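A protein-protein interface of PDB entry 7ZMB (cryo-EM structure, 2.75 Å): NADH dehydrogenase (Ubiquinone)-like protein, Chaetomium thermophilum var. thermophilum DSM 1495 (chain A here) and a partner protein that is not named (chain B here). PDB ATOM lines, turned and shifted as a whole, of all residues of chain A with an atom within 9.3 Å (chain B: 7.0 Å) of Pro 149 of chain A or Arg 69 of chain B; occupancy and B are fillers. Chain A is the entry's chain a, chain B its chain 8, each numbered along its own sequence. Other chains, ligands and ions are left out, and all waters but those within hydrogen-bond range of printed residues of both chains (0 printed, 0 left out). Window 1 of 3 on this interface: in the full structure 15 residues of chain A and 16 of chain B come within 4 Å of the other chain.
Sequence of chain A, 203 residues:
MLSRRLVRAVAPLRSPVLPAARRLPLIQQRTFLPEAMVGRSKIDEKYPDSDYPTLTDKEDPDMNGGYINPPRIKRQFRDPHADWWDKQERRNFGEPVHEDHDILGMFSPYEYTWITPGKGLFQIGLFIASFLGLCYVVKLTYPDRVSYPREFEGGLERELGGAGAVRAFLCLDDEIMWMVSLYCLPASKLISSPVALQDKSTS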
ATOM      1  N   ARG A 145      25.179 -12.026 -15.681  1.00  0.00           N
ATOM      2  CA  ARG A 145      23.811 -11.603 -15.422  1.00  0.00           C
ATOM      3  C   ARG A 145      23.571 -11.441 -13.925  1.00  0.00           C
ATOM      4  O   ARG A 145      24.131 -12.165 -13.098  1.00  0.00           O
ATOM      5  CB  ARG A 145      22.820 -12.603 -16.017  1.00  0.00           C
ATOM      6  CG  ARG A 145      22.820 -13.966 -15.350  1.00  0.00           C
ATOM      7  CD  ARG A 145      22.156 -15.003 -16.239  1.00  0.00           C
ATOM      8  NE  ARG A 145      20.991 -14.464 -16.937  1.00  0.00           N
ATOM      9  CZ  ARG A 145      19.816 -14.224 -16.362  1.00  0.00           C
ATOM     10  NH1 ARG A 145      18.816 -13.732 -17.078  1.00  0.00           N
ATOM     11  NH2 ARG A 145      19.641 -14.474 -15.073  1.00  0.00           N
ATOM     12  N   VAL A 146      22.732 -10.469 -13.581  1.00  0.00           N
ATOM     13  CA  VAL A 146      22.452 -10.113 -12.196  1.00  0.00           C
ATOM     14  C   VAL A 146      21.136 -10.716 -11.721  1.00  0.00           C
ATOM     15  O   VAL A 146      21.074 -11.334 -10.657  1.00  0.00           O
ATOM     16  CB  VAL A 146      22.455  -8.580 -12.010  1.00  0.00           C
ATOM     17  CG1 VAL A 146      22.057  -8.219 -10.592  1.00  0.00           C
ATOM     18  CG2 VAL A 146      23.822  -8.011 -12.340  1.00  0.00           C
ATOM     19  N   SER A 147      20.073 -10.545 -12.496  1.00  0.00           N
ATOM     20  CA  SER A 147      18.747 -10.991 -12.096  1.00  0.00           C
ATOM     21  C   SER A 147      18.451 -12.383 -12.638  1.00  0.00           C
ATOM     22  O   SER A 147      18.883 -12.741 -13.737  1.00  0.00           O
ATOM     23  CB  SER A 147      17.685 -10.005 -12.584  1.00  0.00           C
ATOM     24  OG  SER A 147      17.557 -10.050 -13.994  1.00  0.00           O
ATOM     25  N   TYR A 148      17.704 -13.127 -11.820  1.00  0.00           N
ATOM     26  CA  TYR A 148      17.285 -14.487 -12.218  1.00  0.00           C
ATOM     27  C   TYR A 148      16.176 -14.344 -13.262  1.00  0.00           C
ATOM     28  O   TYR A 148      15.703 -13.234 -13.367  1.00  0.00           O
ATOM     29  CB  TYR A 148      16.775 -15.230 -10.980  1.00  0.00           C
ATOM     30  CG  TYR A 148      16.553 -16.712 -11.150  1.00  0.00           C
ATOM     31  CD1 TYR A 148      17.619 -17.588 -11.244  1.00  0.00           C
ATOM     32  CD2 TYR A 148      15.276 -17.243 -11.192  1.00  0.00           C
ATOM     33  CE1 TYR A 148      17.423 -18.949 -11.394  1.00  0.00           C
ATOM     34  CE2 TYR A 148      15.062 -18.602 -11.341  1.00  0.00           C
ATOM     35  CZ  TYR A 148      16.140 -19.460 -11.442  1.00  0.00           C
ATOM     36  OH  TYR A 148      15.940 -20.803 -11.588  1.00  0.00           O
ATOM     37  N   PRO A 149      15.947 -15.284 -14.204  1.00  0.00           N
ATOM     38  CA  PRO A 149      14.764 -15.264 -15.070  1.00  0.00           C
ATOM     39  C   PRO A 149      13.498 -15.192 -14.233  1.00  0.00           C
ATOM     40  O   PRO A 149      13.397 -15.809 -13.172  1.00  0.00           O
ATOM     41  CB  PRO A 149      14.853 -16.587 -15.840  1.00  0.00           C
ATOM     42  CG  PRO A 149      16.250 -17.071 -15.678  1.00  0.00           C
ATOM     43  CD  PRO A 149      16.958 -16.259 -14.643  1.00  0.00           C
ATOM     44  N   ARG A 150      12.529 -14.420 -14.714  1.00  0.00           N
ATOM     45  CA  ARG A 150      11.307 -14.215 -13.953  1.00  0.00           C
ATOM     46  C   ARG A 150      10.536 -15.519 -13.814  1.00  0.00           C
ATOM     47  O   ARG A 150      10.445 -16.312 -14.754  1.00  0.00           O
ATOM     48  CB  ARG A 150      10.435 -13.154 -14.622  1.00  0.00           C
ATOM     49  CG  ARG A 150      11.202 -11.935 -15.100  1.00  0.00           C
ATOM     50  CD  ARG A 150      10.257 -10.803 -15.453  1.00  0.00           C
ATOM     51  NE  ARG A 150       9.737 -10.141 -14.262  1.00  0.00           N
ATOM     52  CZ  ARG A 150       8.446 -10.043 -13.965  1.00  0.00           C
ATOM     53  NH1 ARG A 150       8.063  -9.420 -12.859  1.00  0.00           N
ATOM     54  NH2 ARG A 150       7.538 -10.567 -14.773  1.00  0.00           N
ATOM     55  N   GLU A 151       9.990 -15.743 -12.624  1.00  0.00           N
ATOM     56  CA  GLU A 151       9.187 -16.923 -12.342  1.00  0.00           C
ATOM     57  C   GLU A 151       7.718 -16.556 -12.498  1.00  0.00           C
ATOM     58  O   GLU A 151       7.223 -15.650 -11.819  1.00  0.00           O
ATOM     59  CB  GLU A 151       9.467 -17.455 -10.938  1.00  0.00           C
ATOM     60  CG  GLU A 151       8.738 -18.747 -10.608  1.00  0.00           C
ATOM     61  CD  GLU A 151       9.295 -19.940 -11.359  1.00  0.00           C
ATOM     62  OE1 GLU A 151      10.460 -19.875 -11.805  1.00  0.00           O
ATOM     63  OE2 GLU A 151       8.567 -20.946 -11.502  1.00  0.00           O
ATOM     64  N   PHE A 152       7.028 -17.255 -13.391  1.00  0.00           N
ATOM     65  CA  PHE A 152       5.617 -17.025 -13.659  1.00  0.00           C
ATOM     66  C   PHE A 152       4.817 -18.215 -13.154  1.00  0.00           C
ATOM     67  O   PHE A 152       5.097 -19.358 -13.528  1.00  0.00           O
ATOM     68  CB  PHE A 152       5.374 -16.821 -15.152  1.00  0.00           C
ATOM     69  CG  PHE A 152       5.863 -15.504 -15.673  1.00  0.00           C
ATOM     70  CD1 PHE A 152       5.102 -14.359 -15.525  1.00  0.00           C
ATOM     71  CD2 PHE A 152       7.085 -15.412 -16.319  1.00  0.00           C
ATOM     72  CE1 PHE A 152       5.550 -13.147 -16.007  1.00  0.00           C
ATOM     73  CE2 PHE A 152       7.538 -14.203 -16.803  1.00  0.00           C
ATOM     74  CZ  PHE A 152       6.770 -13.069 -16.646  1.00  0.00           C
ATOM     75  N   ALA A 168       6.548 -19.741 -20.767  1.00  0.00           N
ATOM     76  CA  ALA A 168       7.381 -18.921 -19.905  1.00  0.00           C
ATOM     77  C   ALA A 168       8.290 -19.819 -19.068  1.00  0.00           C
ATOM     78  O   ALA A 168       8.351 -21.036 -19.260  1.00  0.00           O
ATOM     79  CB  ALA A 168       6.513 -18.018 -19.034  1.00  0.00           C
ATOM     80  N   PHE A 169       9.010 -19.222 -18.122  1.00  0.00           N
ATOM     81  CA  PHE A 169       9.912 -19.960 -17.253  1.00  0.00           C
ATOM     82  C   PHE A 169       9.167 -20.381 -15.993  1.00  0.00           C
ATOM     83  O   PHE A 169       8.577 -19.542 -15.304  1.00  0.00           O
ATOM     84  CB  PHE A 169      11.129 -19.107 -16.894  1.00  0.00           C
ATOM     85  CG  PHE A 169      12.132 -19.812 -16.031  1.00  0.00           C
ATOM     86  CD1 PHE A 169      12.982 -20.761 -16.571  1.00  0.00           C
ATOM     87  CD2 PHE A 169      12.222 -19.532 -14.679  1.00  0.00           C
ATOM     88  CE1 PHE A 169      13.908 -21.414 -15.780  1.00  0.00           C
ATOM     89  CE2 PHE A 169      13.143 -20.184 -13.883  1.00  0.00           C
ATOM     90  CZ  PHE A 169      13.987 -21.126 -14.434  1.00  0.00           C
ATOM     91  N   LEU A 170       9.193 -21.682 -15.695  1.00  0.00           N
ATOM     92  CA  LEU A 170       8.480 -22.207 -14.527  1.00  0.00           C
ATOM     93  C   LEU A 170       9.271 -23.403 -13.986  1.00  0.00           C
ATOM     94  O   LEU A 170       9.114 -24.531 -14.458  1.00  0.00           O
ATOM     95  CB  LEU A 170       7.050 -22.590 -14.878  1.00  0.00           C
ATOM     96  CG  LEU A 170       6.246 -23.323 -13.801  1.00  0.00           C
ATOM     97  CD1 LEU A 170       5.862 -22.378 -12.676  1.00  0.00           C
ATOM     98  CD2 LEU A 170       5.010 -23.972 -14.404  1.00  0.00           C
ATOM     99  N   CYS A 171      10.118 -23.131 -12.991  1.00  0.00           N
ATOM    100  CA  CYS A 171      10.859 -24.166 -12.267  1.00  0.00           C
ATOM    101  C   CYS A 171      11.648 -25.069 -13.213  1.00  0.00           C
ATOM    102  O   CYS A 171      11.714 -26.287 -13.036  1.00  0.00           O
ATOM    103  CB  CYS A 171       9.920 -24.991 -11.388  1.00  0.00           C
ATOM    104  SG  CYS A 171       8.703 -24.013 -10.480  1.00  0.00           S
ATOM    105  N   LEU A 172      12.255 -24.466 -14.229  1.00  0.00           N
ATOM    106  CA  LEU A 172      13.060 -25.194 -15.195  1.00  0.00           C
ATOM    107  C   LEU A 172      14.534 -25.108 -14.808  1.00  0.00           C
ATOM    108  O   LEU A 172      14.894 -24.603 -13.741  1.00  0.00           O
ATOM    109  CB  LEU A 172      12.818 -24.650 -16.603  1.00  0.00           C
ATOM    110  CG  LEU A 172      11.373 -24.586 -17.097  1.00  0.00           C
ATOM    111  CD1 LEU A 172      11.309 -23.867 -18.435  1.00  0.00           C
ATOM    112  CD2 LEU A 172      10.777 -25.980 -17.205  1.00  0.00           C
ATOM    113  N   ASP A 173      15.401 -25.604 -15.685  1.00  0.00           N
ATOM    114  CA  ASP A 173      16.831 -25.497 -15.463  1.00  0.00           C
ATOM    115  C   ASP A 173      17.302 -24.069 -15.731  1.00  0.00           C
ATOM    116  O   ASP A 173      16.585 -23.240 -16.295  1.00  0.00           O
ATOM    117  CB  ASP A 173      17.587 -26.487 -16.348  1.00  0.00           C
ATOM    118  CG  ASP A 173      17.193 -26.380 -17.805  1.00  0.00           C
ATOM    119  OD1 ASP A 173      16.217 -25.661 -18.106  1.00  0.00           O
ATOM    120  OD2 ASP A 173      17.859 -27.015 -18.650  1.00  0.00           O
ATOM    121  N   ASP A 174      18.531 -23.787 -15.314  1.00  0.00           N
ATOM    122  CA  ASP A 174      19.089 -22.448 -15.452  1.00  0.00           C
ATOM    123  C   ASP A 174      20.600 -22.487 -15.654  1.00  0.00           C
ATOM    124  O   ASP A 174      21.226 -21.461 -15.919  1.00  0.00           O
ATOM    125  CB  ASP A 174      18.744 -21.607 -14.223  1.00  0.00           C
ATOM    126  CG  ASP A 174      18.974 -22.357 -12.928  1.00  0.00           C
ATOM    127  OD1 ASP A 174      19.337 -23.549 -12.990  1.00  0.00           O
ATOM    128  OD2 ASP A 174      18.789 -21.759 -11.848  1.00  0.00           O
ATOM    129  N   ASP B  28       2.940 -11.564 -13.794  1.00  0.00           N
ATOM    130  CA  ASP B  28       3.507 -12.191 -12.614  1.00  0.00           C
ATOM    131  C   ASP B  28       2.585 -12.015 -11.408  1.00  0.00           C
ATOM    132  O   ASP B  28       1.610 -11.259 -11.433  1.00  0.00           O
ATOM    133  CB  ASP B  28       4.892 -11.614 -12.314  1.00  0.00           C
ATOM    134  CG  ASP B  28       4.865 -10.115 -12.079  1.00  0.00           C
ATOM    135  OD1 ASP B  28       3.791  -9.498 -12.230  1.00  0.00           O
ATOM    136  OD2 ASP B  28       5.926  -9.552 -11.735  1.00  0.00           O
ATOM    137  N   GLN B  62       7.848  -4.755  -7.032  1.00  0.00           N
ATOM    138  CA  GLN B  62       8.880  -5.110  -8.000  1.00  0.00           C
ATOM    139  C   GLN B  62      10.270  -5.001  -7.383  1.00  0.00           C
ATOM    140  O   GLN B  62      11.112  -5.889  -7.557  1.00  0.00           O
ATOM    141  CB  GLN B  62       8.768  -4.219  -9.237  1.00  0.00           C
ATOM    142  CG  GLN B  62       7.531  -4.475 -10.081  1.00  0.00           C
ATOM    143  CD  GLN B  62       7.563  -5.823 -10.770  1.00  0.00           C
ATOM    144  OE1 GLN B  62       8.338  -6.039 -11.702  1.00  0.00           O
ATOM    145  NE2 GLN B  62       6.715  -6.739 -10.318  1.00  0.00           N
ATOM    146  N   TYR B  63      10.528  -3.911  -6.654  1.00  0.00           N
ATOM    147  CA  TYR B  63      11.837  -3.729  -6.035  1.00  0.00           C
ATOM    148  C   TYR B  63      12.086  -4.767  -4.950  1.00  0.00           C
ATOM    149  O   TYR B  63      13.182  -5.333  -4.867  1.00  0.00           O
ATOM    150  CB  TYR B  63      11.954  -2.317  -5.467  1.00  0.00           C
ATOM    151  CG  TYR B  63      13.292  -2.003  -4.843  1.00  0.00           C
ATOM    152  CD1 TYR B  63      14.406  -1.747  -5.631  1.00  0.00           C
ATOM    153  CD2 TYR B  63      13.440  -1.955  -3.464  1.00  0.00           C
ATOM    154  CE1 TYR B  63      15.630  -1.455  -5.062  1.00  0.00           C
ATOM    155  CE2 TYR B  63      14.659  -1.665  -2.887  1.00  0.00           C
ATOM    156  CZ  TYR B  63      15.750  -1.416  -3.689  1.00  0.00           C
ATOM    157  OH  TYR B  63      16.966  -1.126  -3.116  1.00  0.00           O
ATOM    158  N   LEU B  64      11.085  -5.028  -4.108  1.00  0.00           N
ATOM    159  CA  LEU B  64      11.238  -6.050  -3.078  1.00  0.00           C
ATOM    160  C   LEU B  64      11.440  -7.426  -3.697  1.00  0.00           C
ATOM    161  O   LEU B  64      12.257  -8.219  -3.214  1.00  0.00           O
ATOM    162  CB  LEU B  64      10.024  -6.049  -2.150  1.00  0.00           C
ATOM    163  CG  LEU B  64       9.831  -4.796  -1.297  1.00  0.00           C
ATOM    164  CD1 LEU B  64       8.521  -4.867  -0.531  1.00  0.00           C
ATOM    165  CD2 LEU B  64      11.002  -4.605  -0.349  1.00  0.00           C
ATOM    166  N   GLU B  65      10.699  -7.728  -4.765  1.00  0.00           N
ATOM    167  CA  GLU B  65      10.896  -8.992  -5.466  1.00  0.00           C
ATOM    168  C   GLU B  65      12.290  -9.073  -6.075  1.00  0.00           C
ATOM    169  O   GLU B  65      12.933 -10.127  -6.031  1.00  0.00           O
ATOM    170  CB  GLU B  65       9.832  -9.165  -6.549  1.00  0.00           C
ATOM    171  CG  GLU B  65       9.928 -10.477  -7.310  1.00  0.00           C
ATOM    172  CD  GLU B  65       9.662 -11.682  -6.433  1.00  0.00           C
ATOM    173  OE1 GLU B  65       8.951 -11.537  -5.415  1.00  0.00           O
ATOM    174  OE2 GLU B  65      10.164 -12.778  -6.760  1.00  0.00           O
ATOM    175  N   PHE B  66      12.776  -7.963  -6.634  1.00  0.00           N
ATOM    176  CA  PHE B  66      14.080  -7.970  -7.290  1.00  0.00           C
ATOM    177  C   PHE B  66      15.192  -8.337  -6.317  1.00  0.00           C
ATOM    178  O   PHE B  66      16.085  -9.124  -6.654  1.00  0.00           O
ATOM    179  CB  PHE B  66      14.349  -6.604  -7.920  1.00  0.00           C
ATOM    180  CG  PHE B  66      15.667  -6.516  -8.629  1.00  0.00           C
ATOM    181  CD1 PHE B  66      16.041  -7.482  -9.545  1.00  0.00           C
ATOM    182  CD2 PHE B  66      16.535  -5.468  -8.375  1.00  0.00           C
ATOM    183  CE1 PHE B  66      17.255  -7.402 -10.197  1.00  0.00           C
ATOM    184  CE2 PHE B  66      17.751  -5.383  -9.023  1.00  0.00           C
ATOM    185  CZ  PHE B  66      18.111  -6.352  -9.935  1.00  0.00           C
ATOM    186  N   LYS B  67      15.159  -7.777  -5.106  1.00  0.00           N
ATOM    187  CA  LYS B  67      16.197  -8.087  -4.128  1.00  0.00           C
ATOM    188  C   LYS B  67      16.145  -9.548  -3.705  1.00  0.00           C
ATOM    189  O   LYS B  67      17.189 -10.187  -3.531  1.00  0.00           O
ATOM    190  CB  LYS B  67      16.077  -7.163  -2.919  1.00  0.00           C
ATOM    191  CG  LYS B  67      16.269  -5.703  -3.271  1.00  0.00           C
ATOM    192  CD  LYS B  67      17.705  -5.456  -3.708  1.00  0.00           C
ATOM    193  CE  LYS B  67      17.958  -3.991  -3.998  1.00  0.00           C
ATOM    194  NZ  LYS B  67      19.349  -3.747  -4.467  1.00  0.00           N
ATOM    195  N   LYS B  68      14.942 -10.098  -3.535  1.00  0.00           N
ATOM    196  CA  LYS B  68      14.823 -11.525  -3.255  1.00  0.00           C
ATOM    197  C   LYS B  68      15.385 -12.350  -4.404  1.00  0.00           C
ATOM    198  O   LYS B  68      16.008 -13.396  -4.186  1.00  0.00           O
ATOM    199  CB  LYS B  68      13.361 -11.890  -2.997  1.00  0.00           C
ATOM    200  CG  LYS B  68      12.787 -11.304  -1.718  1.00  0.00           C
ATOM    201  CD  LYS B  68      11.351 -11.754  -1.510  1.00  0.00           C
ATOM    202  CE  LYS B  68      10.766 -11.171  -0.235  1.00  0.00           C
ATOM    203  NZ  LYS B  68       9.357 -11.609  -0.030  1.00  0.00           N
ATOM    204  N   ARG B  69      15.170 -11.891  -5.636  1.00  0.00           N
ATOM    205  CA  ARG B  69      15.677 -12.596  -6.809  1.00  0.00           C
ATOM    206  C   ARG B  69      17.199 -12.532  -6.888  1.00  0.00           C
ATOM    207  O   ARG B  69      17.862 -13.558  -7.075  1.00  0.00           O
ATOM    208  CB  ARG B  69      15.038 -12.005  -8.063  1.00  0.00           C
ATOM    209  CG  ARG B  69      13.544 -12.259  -8.155  1.00  0.00           C
ATOM    210  CD  ARG B  69      12.951 -11.622  -9.390  1.00  0.00           C
ATOM    211  NE  ARG B  69      13.428 -12.220 -10.627  1.00  0.00           N
ATOM    212  CZ  ARG B  69      13.169 -11.720 -11.828  1.00  0.00           C
ATOM    213  NH1 ARG B  69      13.641 -12.309 -12.914  1.00  0.00           N
ATOM    214  NH2 ARG B  69      12.430 -10.628 -11.941  1.00  0.00           N
ATOM    215  N   VAL B  70      17.771 -11.334  -6.744  1.00  0.00           N
ATOM    216  CA  VAL B  70      19.219 -11.197  -6.878  1.00  0.00           C
ATOM    217  C   VAL B  70      19.938 -11.880  -5.722  1.00  0.00           C
ATOM    218  O   VAL B  70      21.028 -12.438  -5.903  1.00  0.00           O
ATOM    219  CB  VAL B  70      19.616  -9.714  -7.007  1.00  0.00           C
ATOM    220  CG1 VAL B  70      19.252  -8.940  -5.755  1.00  0.00           C
ATOM    221  CG2 VAL B  70      21.101  -9.585  -7.305  1.00  0.00           C
ATOM    222  N   GLN B  71      19.352 -11.856  -4.521  1.00  0.00           N
ATOM    223  CA  GLN B  71      19.956 -12.535  -3.380  1.00  0.00           C
ATOM    224  C   GLN B  71      20.006 -14.043  -3.573  1.00  0.00           C
ATOM    225  O   GLN B  71      20.797 -14.719  -2.905  1.00  0.00           O
ATOM    226  CB  GLN B  71      19.188 -12.198  -2.099  1.00  0.00           C
ATOM    227  CG  GLN B  71      19.907 -12.586  -0.815  1.00  0.00           C
ATOM    228  CD  GLN B  71      19.000 -12.531   0.397  1.00  0.00           C
ATOM    229  OE1 GLN B  71      17.800 -12.289   0.278  1.00  0.00           O
ATOM    230  NE2 GLN B  71      19.572 -12.750   1.576  1.00  0.00           N
ATOM    231  N   LYS B  72      19.166 -14.560  -4.480  1.00  0.00           N
ATOM    232  CA  LYS B  72      19.142 -16.020  -4.775  1.00  0.00           C
ATOM    233  C   LYS B  72      20.422 -16.396  -5.524  1.00  0.00           C
ATOM    234  O   LYS B  72      20.910 -17.524  -5.341  1.00  0.00           O
ATOM    235  CB  LYS B  72      17.906 -16.373  -5.607  1.00  0.00           C
ATOM    236  CG  LYS B  72      17.802 -17.824  -6.056  1.00  0.00           C
ATOM    237  CD  LYS B  72      16.832 -18.027  -7.199  1.00  0.00           C
ATOM    238  CE  LYS B  72      15.441 -17.517  -6.894  1.00  0.00           C
ATOM    239  NZ  LYS B  72      14.510 -17.756  -8.022  1.00  0.00           N
ATOM    240  N   MET B  73      20.943 -15.488  -6.350  1.00  0.00           N
ATOM    241  CA  MET B  73      22.206 -15.760  -7.029  1.00  0.00           C
ATOM    242  C   MET B  73      23.359 -15.973  -6.059  1.00  0.00           C
ATOM    243  O   MET B  73      24.356 -16.594  -6.438  1.00  0.00           O
ATOM    244  CB  MET B  73      22.573 -14.615  -7.973  1.00  0.00           C
ATOM    245  CG  MET B  73      21.652 -14.403  -9.149  1.00  0.00           C
ATOM    246  SD  MET B  73      21.685 -15.828 -10.246  1.00  0.00           S
ATOM    247  CE  MET B  73      20.379 -15.398 -11.369  1.00  0.00           C
ATOM    248  N   GLU B  74      23.247 -15.471  -4.827  1.00  0.00           N
ATOM    249  CA  GLU B  74      24.353 -15.560  -3.879  1.00  0.00           C
ATOM    250  C   GLU B  74      24.763 -17.007  -3.642  1.00  0.00           C
ATOM    251  O   GLU B  74      25.953 -17.315  -3.515  1.00  0.00           O
ATOM    252  CB  GLU B  74      23.969 -14.883  -2.563  1.00  0.00           C
ATOM    253  CG  GLU B  74      23.702 -13.396  -2.701  1.00  0.00           C
ATOM    254  CD  GLU B  74      24.908 -12.639  -3.214  1.00  0.00           C
ATOM    255  OE1 GLU B  74      26.037 -12.951  -2.780  1.00  0.00           O
ATOM    256  OE2 GLU B  74      24.730 -11.740  -4.063  1.00  0.00           O
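OD2 of Asp 28 of chain B is in salt-bridge range of NH1 of Arg 150 of chain A, 2.4 Å away.
The backbone carbonyl oxygen (O) of Tyr 148 of chain A sits close to the guanidinium group (NH1) of Arg 69 of chain B, 2.3 Å away.
NH1 of Arg 69 of chain B sits close to N of Arg 150 of chain A, at 3.0 Å.
The guanidinium group (NH1) of Arg 145 of chain A sits close to the backbone carbonyl oxygen (O) of Ser 147 of chain A.
OD2 of Asp 174 of chain A is in hydrogen-bond range of OH of Tyr 148 of chain A (3.0 Å).
N of Phe 152 of chain A sits at hydrogen-bond distance from O of Phe 169 of chain A (3.4 Å).
OD2 of Asp 28 of chain B is in hydrogen-bond range of NE2 of Gln 62 of chain B, at 3.2 Å.
Among the printed residues, pairs that only touch across the chains: Pro 149 of chain A with Arg 69 of chain B (3.2 Å), Tyr 148 of chain A with Lys 72 of chain B (3.3 Å), Tyr 148 of chain A with Met 73 of chain B (3.3 Å), Val 146 of chain A with Met 73 of chain B (3.5 Å), Ser 147 of chain A with Phe 66 of chain B (3.6 Å), Arg 150 of chain A with Gln 62 of chain B (3.6 Å), Val 146 of chain A with Val 70 of chain B (3.7 Å), Phe 152 of chain A with Asp 28 of chain B (3.8 Å), Ser 147 of chain A with Met 73 of chain B (3.8 Å) and Arg 145 of chain A with Met 73 of chain B (3.9 Å).
Of the printed residues of chain B, Val 146 of chain A touches Val 70 and Met 73.
Of the printed residues of chain B, Ser 147 of chain A touches Phe 66 and Met 73.
Pro 149 of chain A touches one residue of chain B.
Printed residues of chain B within 4 Å of Arg 150 of chain A: Asp 28 (2.4 Å), Gln 62 (3.6 Å) and Arg 69 (3.0 Å).
Glu 151 of chain A touches none of the printed residues of chain B.
Leu 64 of chain B touches none of the printed residues of chain A.
Of the printed residues of chain A, Arg 69 of chain B touches Tyr 148, Pro 149 and Arg 150.
Of chain A, only Val 146 comes within 4 Å of Val 70 of chain B.
Of the printed residues of chain A, Lys 72 of chain B touches Tyr 148.
The nearest residue of chain A that does not touch Arg 69 of chain B is Ser 147 of chain A (4.6 Å).
Of the 15 printed residues of chain A, 7 touch a printed residue of chain B.
Printed residues of chain A that touch a printed residue of chain B: Arg 145, Val 146, Ser 147, Tyr 148, Pro 149, Arg 150 and Phe 152.
Hydrophobic or aromatic side chains of chain A that line the printed part of chain B: Val 146, Tyr 148 and Phe 152.
Printed residues of chain B that touch a printed residue of chain A: Asp 28, Gln 62, Phe 66, Arg 69, Val 70, Lys 72 and Met 73.
Hydrophobic or aromatic side chains of chain B within 4 Å of the printed part of chain A: Phe 66, Val 70 and Met 73.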
